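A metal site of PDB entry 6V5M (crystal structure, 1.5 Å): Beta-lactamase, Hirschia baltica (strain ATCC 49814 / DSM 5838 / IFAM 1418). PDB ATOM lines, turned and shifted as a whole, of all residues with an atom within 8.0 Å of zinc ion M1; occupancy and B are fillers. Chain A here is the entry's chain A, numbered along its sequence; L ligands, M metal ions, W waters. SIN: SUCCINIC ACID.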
ATOM      1  N   ILE A  43     -22.179  -8.581 -33.472  1.00  0.00           N
ATOM      2  CA  ILE A  43     -21.277  -7.544 -32.956  1.00  0.00           C
ATOM      3  C   ILE A  43     -21.374  -7.538 -31.432  1.00  0.00           C
ATOM      4  O   ILE A  43     -22.477  -7.507 -30.845  1.00  0.00           O
ATOM      5  CB  ILE A  43     -21.536  -6.157 -33.564  1.00  0.00           C
ATOM      6  CG1 ILE A  43     -20.603  -5.126 -32.938  1.00  0.00           C
ATOM      7  CG2 ILE A  43     -22.965  -5.719 -33.415  1.00  0.00           C
ATOM      8  CD1 ILE A  43     -20.556  -3.800 -33.670  1.00  0.00           C
ATOM      9  N   ARG A  44     -20.220  -7.578 -30.784  1.00  0.00           N
ATOM     10  CA  ARG A  44     -20.178  -7.544 -29.322  1.00  0.00           C
ATOM     11  C   ARG A  44     -20.333  -6.122 -28.806  1.00  0.00           C
ATOM     12  O   ARG A  44     -19.994  -5.158 -29.491  1.00  0.00           O
ATOM     13  CB  ARG A  44     -18.844  -8.097 -28.827  1.00  0.00           C
ATOM     14  CG  ARG A  44     -17.704  -7.086 -28.909  1.00  0.00           C
ATOM     15  CD  ARG A  44     -16.382  -7.730 -28.635  1.00  0.00           C
ATOM     16  NE  ARG A  44     -16.275  -8.102 -27.230  1.00  0.00           N
ATOM     17  CZ  ARG A  44     -15.390  -8.963 -26.745  1.00  0.00           C
ATOM     18  NH1 ARG A  44     -14.508  -9.583 -27.539  1.00  0.00           N
ATOM     19  NH2 ARG A  44     -15.398  -9.209 -25.434  1.00  0.00           N
ATOM     20  N   THR A  45     -20.823  -6.007 -27.587  1.00  0.00           N
ATOM     21  CA  THR A  45     -20.717  -4.755 -26.823  1.00  0.00           C
ATOM     22  C   THR A  45     -20.285  -5.117 -25.407  1.00  0.00           C
ATOM     23  O   THR A  45     -20.807  -6.103 -24.855  1.00  0.00           O
ATOM     24  CB  THR A  45     -21.986  -3.857 -26.825  1.00  0.00           C
ATOM     25  OG1 THR A  45     -21.622  -2.607 -26.213  1.00  0.00           O
ATOM     26  CG2 THR A  45     -23.198  -4.449 -26.072  1.00  0.00           C
ATOM     27  N   ASN A  46     -19.314  -4.383 -24.870  1.00  0.00           N
ATOM     28  CA  ASN A  46     -18.746  -4.635 -23.537  1.00  0.00           C
ATOM     29  C   ASN A  46     -19.131  -3.556 -22.538  1.00  0.00           C
ATOM     30  O   ASN A  46     -19.142  -2.357 -22.869  1.00  0.00           O
ATOM     31  CB  ASN A  46     -17.212  -4.646 -23.582  1.00  0.00           C
ATOM     32  CG  ASN A  46     -16.649  -5.651 -24.548  1.00  0.00           C
ATOM     33  OD1 ASN A  46     -17.203  -6.741 -24.736  1.00  0.00           O
ATOM     34  ND2 ASN A  46     -15.550  -5.284 -25.193  1.00  0.00           N
ATOM     35  N   TRP A  63     -27.192  -4.836 -25.078  1.00  0.00           N
ATOM     36  CA  TRP A  63     -27.993  -4.329 -26.196  1.00  0.00           C
ATOM     37  C   TRP A  63     -29.476  -4.204 -25.868  1.00  0.00           C
ATOM     38  O   TRP A  63     -30.177  -3.427 -26.537  1.00  0.00           O
ATOM     39  CB  TRP A  63     -27.855  -5.262 -27.391  1.00  0.00           C
ATOM     40  CG  TRP A  63     -26.527  -5.281 -28.029  1.00  0.00           C
ATOM     41  CD1 TRP A  63     -25.581  -6.282 -27.944  1.00  0.00           C
ATOM     42  CD2 TRP A  63     -26.008  -4.324 -28.965  1.00  0.00           C
ATOM     43  NE1 TRP A  63     -24.494  -5.982 -28.740  1.00  0.00           N
ATOM     44  CE2 TRP A  63     -24.723  -4.788 -29.370  1.00  0.00           C
ATOM     45  CE3 TRP A  63     -26.474  -3.111 -29.475  1.00  0.00           C
ATOM     46  CZ2 TRP A  63     -23.913  -4.082 -30.276  1.00  0.00           C
ATOM     47  CZ3 TRP A  63     -25.655  -2.406 -30.421  1.00  0.00           C
ATOM     48  CH2 TRP A  63     -24.403  -2.901 -30.793  1.00  0.00           C
ATOM     49  N   THR A  89     -22.364   5.397 -20.655  1.00  0.00           N
ATOM     50  CA  THR A  89     -21.246   6.172 -21.207  1.00  0.00           C
ATOM     51  C   THR A  89     -21.568   6.929 -22.497  1.00  0.00           C
ATOM     52  O   THR A  89     -20.764   7.793 -22.880  1.00  0.00           O
ATOM     53  CB  THR A  89     -19.978   5.301 -21.364  1.00  0.00           C
ATOM     54  OG1 THR A  89     -20.220   4.204 -22.263  1.00  0.00           O
ATOM     55  CG2 THR A  89     -19.504   4.787 -19.966  1.00  0.00           C
ATOM     56  N   HIS A  90     -22.733   6.706 -23.117  1.00  0.00           N
ATOM     57  CA  HIS A  90     -23.331   7.645 -24.074  1.00  0.00           C
ATOM     58  C   HIS A  90     -24.689   7.079 -24.490  1.00  0.00           C
ATOM     59  O   HIS A  90     -25.034   5.933 -24.180  1.00  0.00           O
ATOM     60  CB  HIS A  90     -22.458   7.947 -25.304  1.00  0.00           C
ATOM     61  CG  HIS A  90     -22.288   6.776 -26.209  1.00  0.00           C
ATOM     62  ND1 HIS A  90     -21.356   5.791 -25.954  1.00  0.00           N
ATOM     63  CD2 HIS A  90     -22.881   6.441 -27.377  1.00  0.00           C
ATOM     64  CE1 HIS A  90     -21.386   4.892 -26.933  1.00  0.00           C
ATOM     65  NE2 HIS A  90     -22.317   5.251 -27.790  1.00  0.00           N
ATOM     66  N   HIS A  92     -26.493   5.550 -26.857  1.00  0.00           N
ATOM     67  CA  HIS A  92     -26.760   4.615 -27.942  1.00  0.00           C
ATOM     68  C   HIS A  92     -27.259   3.311 -27.345  1.00  0.00           C
ATOM     69  O   HIS A  92     -27.088   3.060 -26.135  1.00  0.00           O
ATOM     70  CB  HIS A  92     -25.531   4.315 -28.830  1.00  0.00           C
ATOM     71  CG  HIS A  92     -25.238   5.367 -29.844  1.00  0.00           C
ATOM     72  ND1 HIS A  92     -23.968   5.544 -30.378  1.00  0.00           N
ATOM     73  CD2 HIS A  92     -26.027   6.289 -30.440  1.00  0.00           C
ATOM     74  CE1 HIS A  92     -24.010   6.509 -31.279  1.00  0.00           C
ATOM     75  NE2 HIS A  92     -25.238   6.982 -31.343  1.00  0.00           N
ATOM     76  N   SER A  93     -27.861   2.477 -28.187  1.00  0.00           N
ATOM     77  CA  SER A  93     -28.580   1.292 -27.686  1.00  0.00           C
ATOM     78  C   SER A  93     -27.637   0.203 -27.155  1.00  0.00           C
ATOM     79  O   SER A  93     -28.092  -0.677 -26.408  1.00  0.00           O
ATOM     80  CB  SER A  93     -29.500   0.731 -28.770  1.00  0.00           C
ATOM     81  OG  SER A  93     -28.752   0.167 -29.830  1.00  0.00           O
ATOM     82  N   ASP A  94     -26.358   0.215 -27.521  1.00  0.00           N
ATOM     83  CA  ASP A  94     -25.446  -0.730 -26.895  1.00  0.00           C
ATOM     84  C   ASP A  94     -25.137  -0.392 -25.441  1.00  0.00           C
ATOM     85  O   ASP A  94     -24.697  -1.263 -24.689  1.00  0.00           O
ATOM     86  CB  ASP A  94     -24.150  -0.963 -27.699  1.00  0.00           C
ATOM     87  CG  ASP A  94     -23.478   0.340 -28.195  1.00  0.00           C
ATOM     88  OD1 ASP A  94     -24.087   1.412 -28.306  1.00  0.00           O
ATOM     89  OD2 ASP A  94     -22.300   0.241 -28.540  1.00  0.00           O
ATOM     90  N   LYS A  95     -25.343   0.861 -25.054  1.00  0.00           N
ATOM     91  CA  LYS A  95     -25.011   1.354 -23.719  1.00  0.00           C
ATOM     92  C   LYS A  95     -26.226   1.584 -22.849  1.00  0.00           C
ATOM     93  O   LYS A  95     -26.104   1.571 -21.618  1.00  0.00           O
ATOM     94  CB  LYS A  95     -24.223   2.686 -23.839  1.00  0.00           C
ATOM     95  CG  LYS A  95     -23.095   2.711 -24.906  1.00  0.00           C
ATOM     96  CD  LYS A  95     -21.771   2.077 -24.438  1.00  0.00           C
ATOM     97  CE  LYS A  95     -21.806   0.542 -24.575  1.00  0.00           C
ATOM     98  NZ  LYS A  95     -20.586  -0.011 -23.892  1.00  0.00           N
ATOM     99  N   HIS A 154     -16.771   9.710 -30.391  1.00  0.00           N
ATOM    100  CA  HIS A 154     -17.711   8.795 -31.022  1.00  0.00           C
ATOM    101  C   HIS A 154     -19.130   9.348 -30.959  1.00  0.00           C
ATOM    102  O   HIS A 154     -19.923   9.199 -31.896  1.00  0.00           O
ATOM    103  CB  HIS A 154     -17.642   7.458 -30.279  1.00  0.00           C
ATOM    104  CG  HIS A 154     -18.813   6.573 -30.545  1.00  0.00           C
ATOM    105  ND1 HIS A 154     -18.913   5.777 -31.680  1.00  0.00           N
ATOM    106  CD2 HIS A 154     -19.967   6.397 -29.856  1.00  0.00           C
ATOM    107  CE1 HIS A 154     -20.054   5.104 -31.638  1.00  0.00           C
ATOM    108  NE2 HIS A 154     -20.716   5.462 -30.543  1.00  0.00           N
ATOM    109  N   GLY A 172     -15.113   2.677 -23.552  1.00  0.00           N
ATOM    110  CA  GLY A 172     -16.389   2.613 -24.253  1.00  0.00           C
ATOM    111  C   GLY A 172     -16.213   2.722 -25.769  1.00  0.00           C
ATOM    112  O   GLY A 172     -15.210   2.277 -26.332  1.00  0.00           O
ATOM    113  N   CYS A 173     -17.202   3.337 -26.414  1.00  0.00           N
ATOM    114  CA  CYS A 173     -17.196   3.413 -27.867  1.00  0.00           C
ATOM    115  C   CYS A 173     -16.276   4.512 -28.379  1.00  0.00           C
ATOM    116  O   CYS A 173     -15.986   4.532 -29.586  1.00  0.00           O
ATOM    117  CB  CYS A 173     -18.615   3.620 -28.405  1.00  0.00           C
ATOM    118  SG  CYS A 173     -19.660   2.268 -27.825  1.00  0.00           S
ATOM    119  N   MET A 174     -15.764   5.397 -27.496  1.00  0.00           N
ATOM    120  CA  MET A 174     -14.781   6.383 -27.920  1.00  0.00           C
ATOM    121  C   MET A 174     -13.449   5.736 -28.282  1.00  0.00           C
ATOM    122  O   MET A 174     -12.673   6.333 -29.036  1.00  0.00           O
ATOM    123  CB  MET A 174     -14.583   7.417 -26.797  1.00  0.00           C
ATOM    124  CG  MET A 174     -13.858   8.709 -27.250  1.00  0.00           C
ATOM    125  SD  MET A 174     -13.554   9.813 -25.904  1.00  0.00           S
ATOM    126  CE  MET A 174     -12.028   9.074 -25.331  1.00  0.00           C
ATOM    127  N   ILE A 175     -13.171   4.515 -27.812  1.00  0.00           N
ATOM    128  CA  ILE A 175     -11.934   3.804 -28.139  1.00  0.00           C
ATOM    129  C   ILE A 175     -12.295   2.667 -29.088  1.00  0.00           C
ATOM    130  O   ILE A 175     -13.135   1.808 -28.761  1.00  0.00           O
ATOM    131  CB  ILE A 175     -11.217   3.308 -26.877  1.00  0.00           C
ATOM    132  CG1 ILE A 175     -10.935   4.478 -25.916  1.00  0.00           C
ATOM    133  CG2 ILE A 175      -9.913   2.596 -27.222  1.00  0.00           C
ATOM    134  CD1 ILE A 175     -10.142   5.682 -26.567  1.00  0.00           C
ATOM    135  N   ARG A 176     -11.676   2.672 -30.267  1.00  0.00           N
ATOM    136  CA  ARG A 176     -11.939   1.683 -31.289  1.00  0.00           C
ATOM    137  C   ARG A 176     -11.135   0.410 -31.016  1.00  0.00           C
ATOM    138  O   ARG A 176     -10.090   0.457 -30.359  1.00  0.00           O
ATOM    139  CB  ARG A 176     -11.588   2.246 -32.678  1.00  0.00           C
ATOM    140  CG  ARG A 176     -12.519   3.447 -33.065  1.00  0.00           C
ATOM    141  CD  ARG A 176     -14.012   3.060 -33.240  1.00  0.00           C
ATOM    142  NE  ARG A 176     -14.135   2.078 -34.321  1.00  0.00           N
ATOM    143  CZ  ARG A 176     -15.037   1.096 -34.395  1.00  0.00           C
ATOM    144  NH1 ARG A 176     -15.940   0.891 -33.430  1.00  0.00           N
ATOM    145  NH2 ARG A 176     -15.011   0.269 -35.443  1.00  0.00           N
ATOM    146  N   GLY A 184     -16.447   2.691 -37.273  1.00  0.00           N
ATOM    147  CA  GLY A 184     -17.686   2.213 -36.670  1.00  0.00           C
ATOM    148  C   GLY A 184     -18.837   3.162 -36.999  1.00  0.00           C
ATOM    149  O   GLY A 184     -18.856   3.827 -38.046  1.00  0.00           O
ATOM    150  N   ASN A 185     -19.816   3.229 -36.081  1.00  0.00           N
ATOM    151  CA  ASN A 185     -20.986   4.072 -36.277  1.00  0.00           C
ATOM    152  C   ASN A 185     -20.628   5.525 -35.975  1.00  0.00           C
ATOM    153  O   ASN A 185     -20.459   5.915 -34.809  1.00  0.00           O
ATOM    154  CB  ASN A 185     -22.129   3.621 -35.367  1.00  0.00           C
ATOM    155  CG  ASN A 185     -23.284   4.582 -35.373  1.00  0.00           C
ATOM    156  OD1 ASN A 185     -23.434   5.375 -36.308  1.00  0.00           O
ATOM    157  ND2 ASN A 185     -24.096   4.543 -34.327  1.00  0.00           N
ATOM    158  N   PRO A 213     -12.298  -1.230 -24.934  1.00  0.00           N
ATOM    159  CA  PRO A 213     -13.215  -0.650 -25.917  1.00  0.00           C
ATOM    160  C   PRO A 213     -14.544  -1.396 -25.869  1.00  0.00           C
ATOM    161  O   PRO A 213     -14.591  -2.561 -25.456  1.00  0.00           O
ATOM    162  CB  PRO A 213     -12.501  -0.960 -27.240  1.00  0.00           C
ATOM    163  CG  PRO A 213     -11.853  -2.389 -26.947  1.00  0.00           C
ATOM    164  CD  PRO A 213     -11.515  -2.368 -25.463  1.00  0.00           C
ATOM    165  N   SER A 214     -15.622  -0.733 -26.279  1.00  0.00           N
ATOM    166  CA  SER A 214     -16.932  -1.415 -26.283  1.00  0.00           C
ATOM    167  C   SER A 214     -16.957  -2.596 -27.249  1.00  0.00           C
ATOM    168  O   SER A 214     -17.608  -3.605 -26.972  1.00  0.00           O
ATOM    169  CB  SER A 214     -18.049  -0.480 -26.713  1.00  0.00           C
ATOM    170  OG  SER A 214     -18.323   0.438 -25.708  1.00  0.00           O
ATOM    171  N   HIS A 215     -16.298  -2.476 -28.410  1.00  0.00           N
ATOM    172  CA  HIS A 215     -16.550  -3.408 -29.514  1.00  0.00           C
ATOM    173  C   HIS A 215     -15.348  -4.269 -29.874  1.00  0.00           C
ATOM    174  O   HIS A 215     -15.261  -4.764 -31.003  1.00  0.00           O
ATOM    175  CB  HIS A 215     -17.130  -2.659 -30.721  1.00  0.00           C
ATOM    176  CG  HIS A 215     -18.386  -1.926 -30.392  1.00  0.00           C
ATOM    177  ND1 HIS A 215     -19.502  -2.563 -29.889  1.00  0.00           N
ATOM    178  CD2 HIS A 215     -18.677  -0.610 -30.432  1.00  0.00           C
ATOM    179  CE1 HIS A 215     -20.452  -1.663 -29.672  1.00  0.00           C
ATOM    180  NE2 HIS A 215     -19.981  -0.461 -29.984  1.00  0.00           N
HETATM  181  C1  SIN L   1     -19.864   1.681 -32.584  1.00  0.00           C
HETATM  182  O1  SIN L   1     -19.732   2.042 -31.361  1.00  0.00           O
HETATM  183  O2  SIN L   1     -19.198   2.303 -33.437  1.00  0.00           O
HETATM  184  C2  SIN L   1     -20.775   0.513 -33.004  1.00  0.00           C
HETATM  185  C3  SIN L   1     -20.714   0.140 -34.504  1.00  0.00           C
HETATM  186  C4  SIN L   1     -19.455  -0.570 -34.978  1.00  0.00           C
HETATM  187  O3  SIN L   1     -18.513  -0.918 -34.233  1.00  0.00           O
HETATM  188  O4  SIN L   1     -19.343  -0.815 -36.193  1.00  0.00           O
HETATM  189 ZN    ZN M   1     -20.857   1.385 -29.609  1.00  0.00          ZN
HETATM  190 ZN    ZN M   2     -22.333   4.574 -29.721  1.00  0.00          ZN
HETATM  191  O   HOH W   1     -22.362   2.660 -30.132  1.00  0.00           O
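ND1 of His 215 sits at hydrogen-bond distance from O of Arg 44 (2.7 Å).
The side-chain hydroxyl (OG) of Ser 214 lies within hydrogen-bond range of the backbone NH (N) of Cys 173 (3.2 Å).
Zinc ion M1 is bound by water W1 (2.0 Å), a ring nitrogen (NE2) of His 215 (2.1 Å), the side-chain carboxylate of Asp 94 (2.1 Å), an oxygen (O1) of the ligand (2.2 Å) and the side-chain sulfur of Cys 173 (2.3 Å).
Zinc ion M1 has five donor atoms within binding distance.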
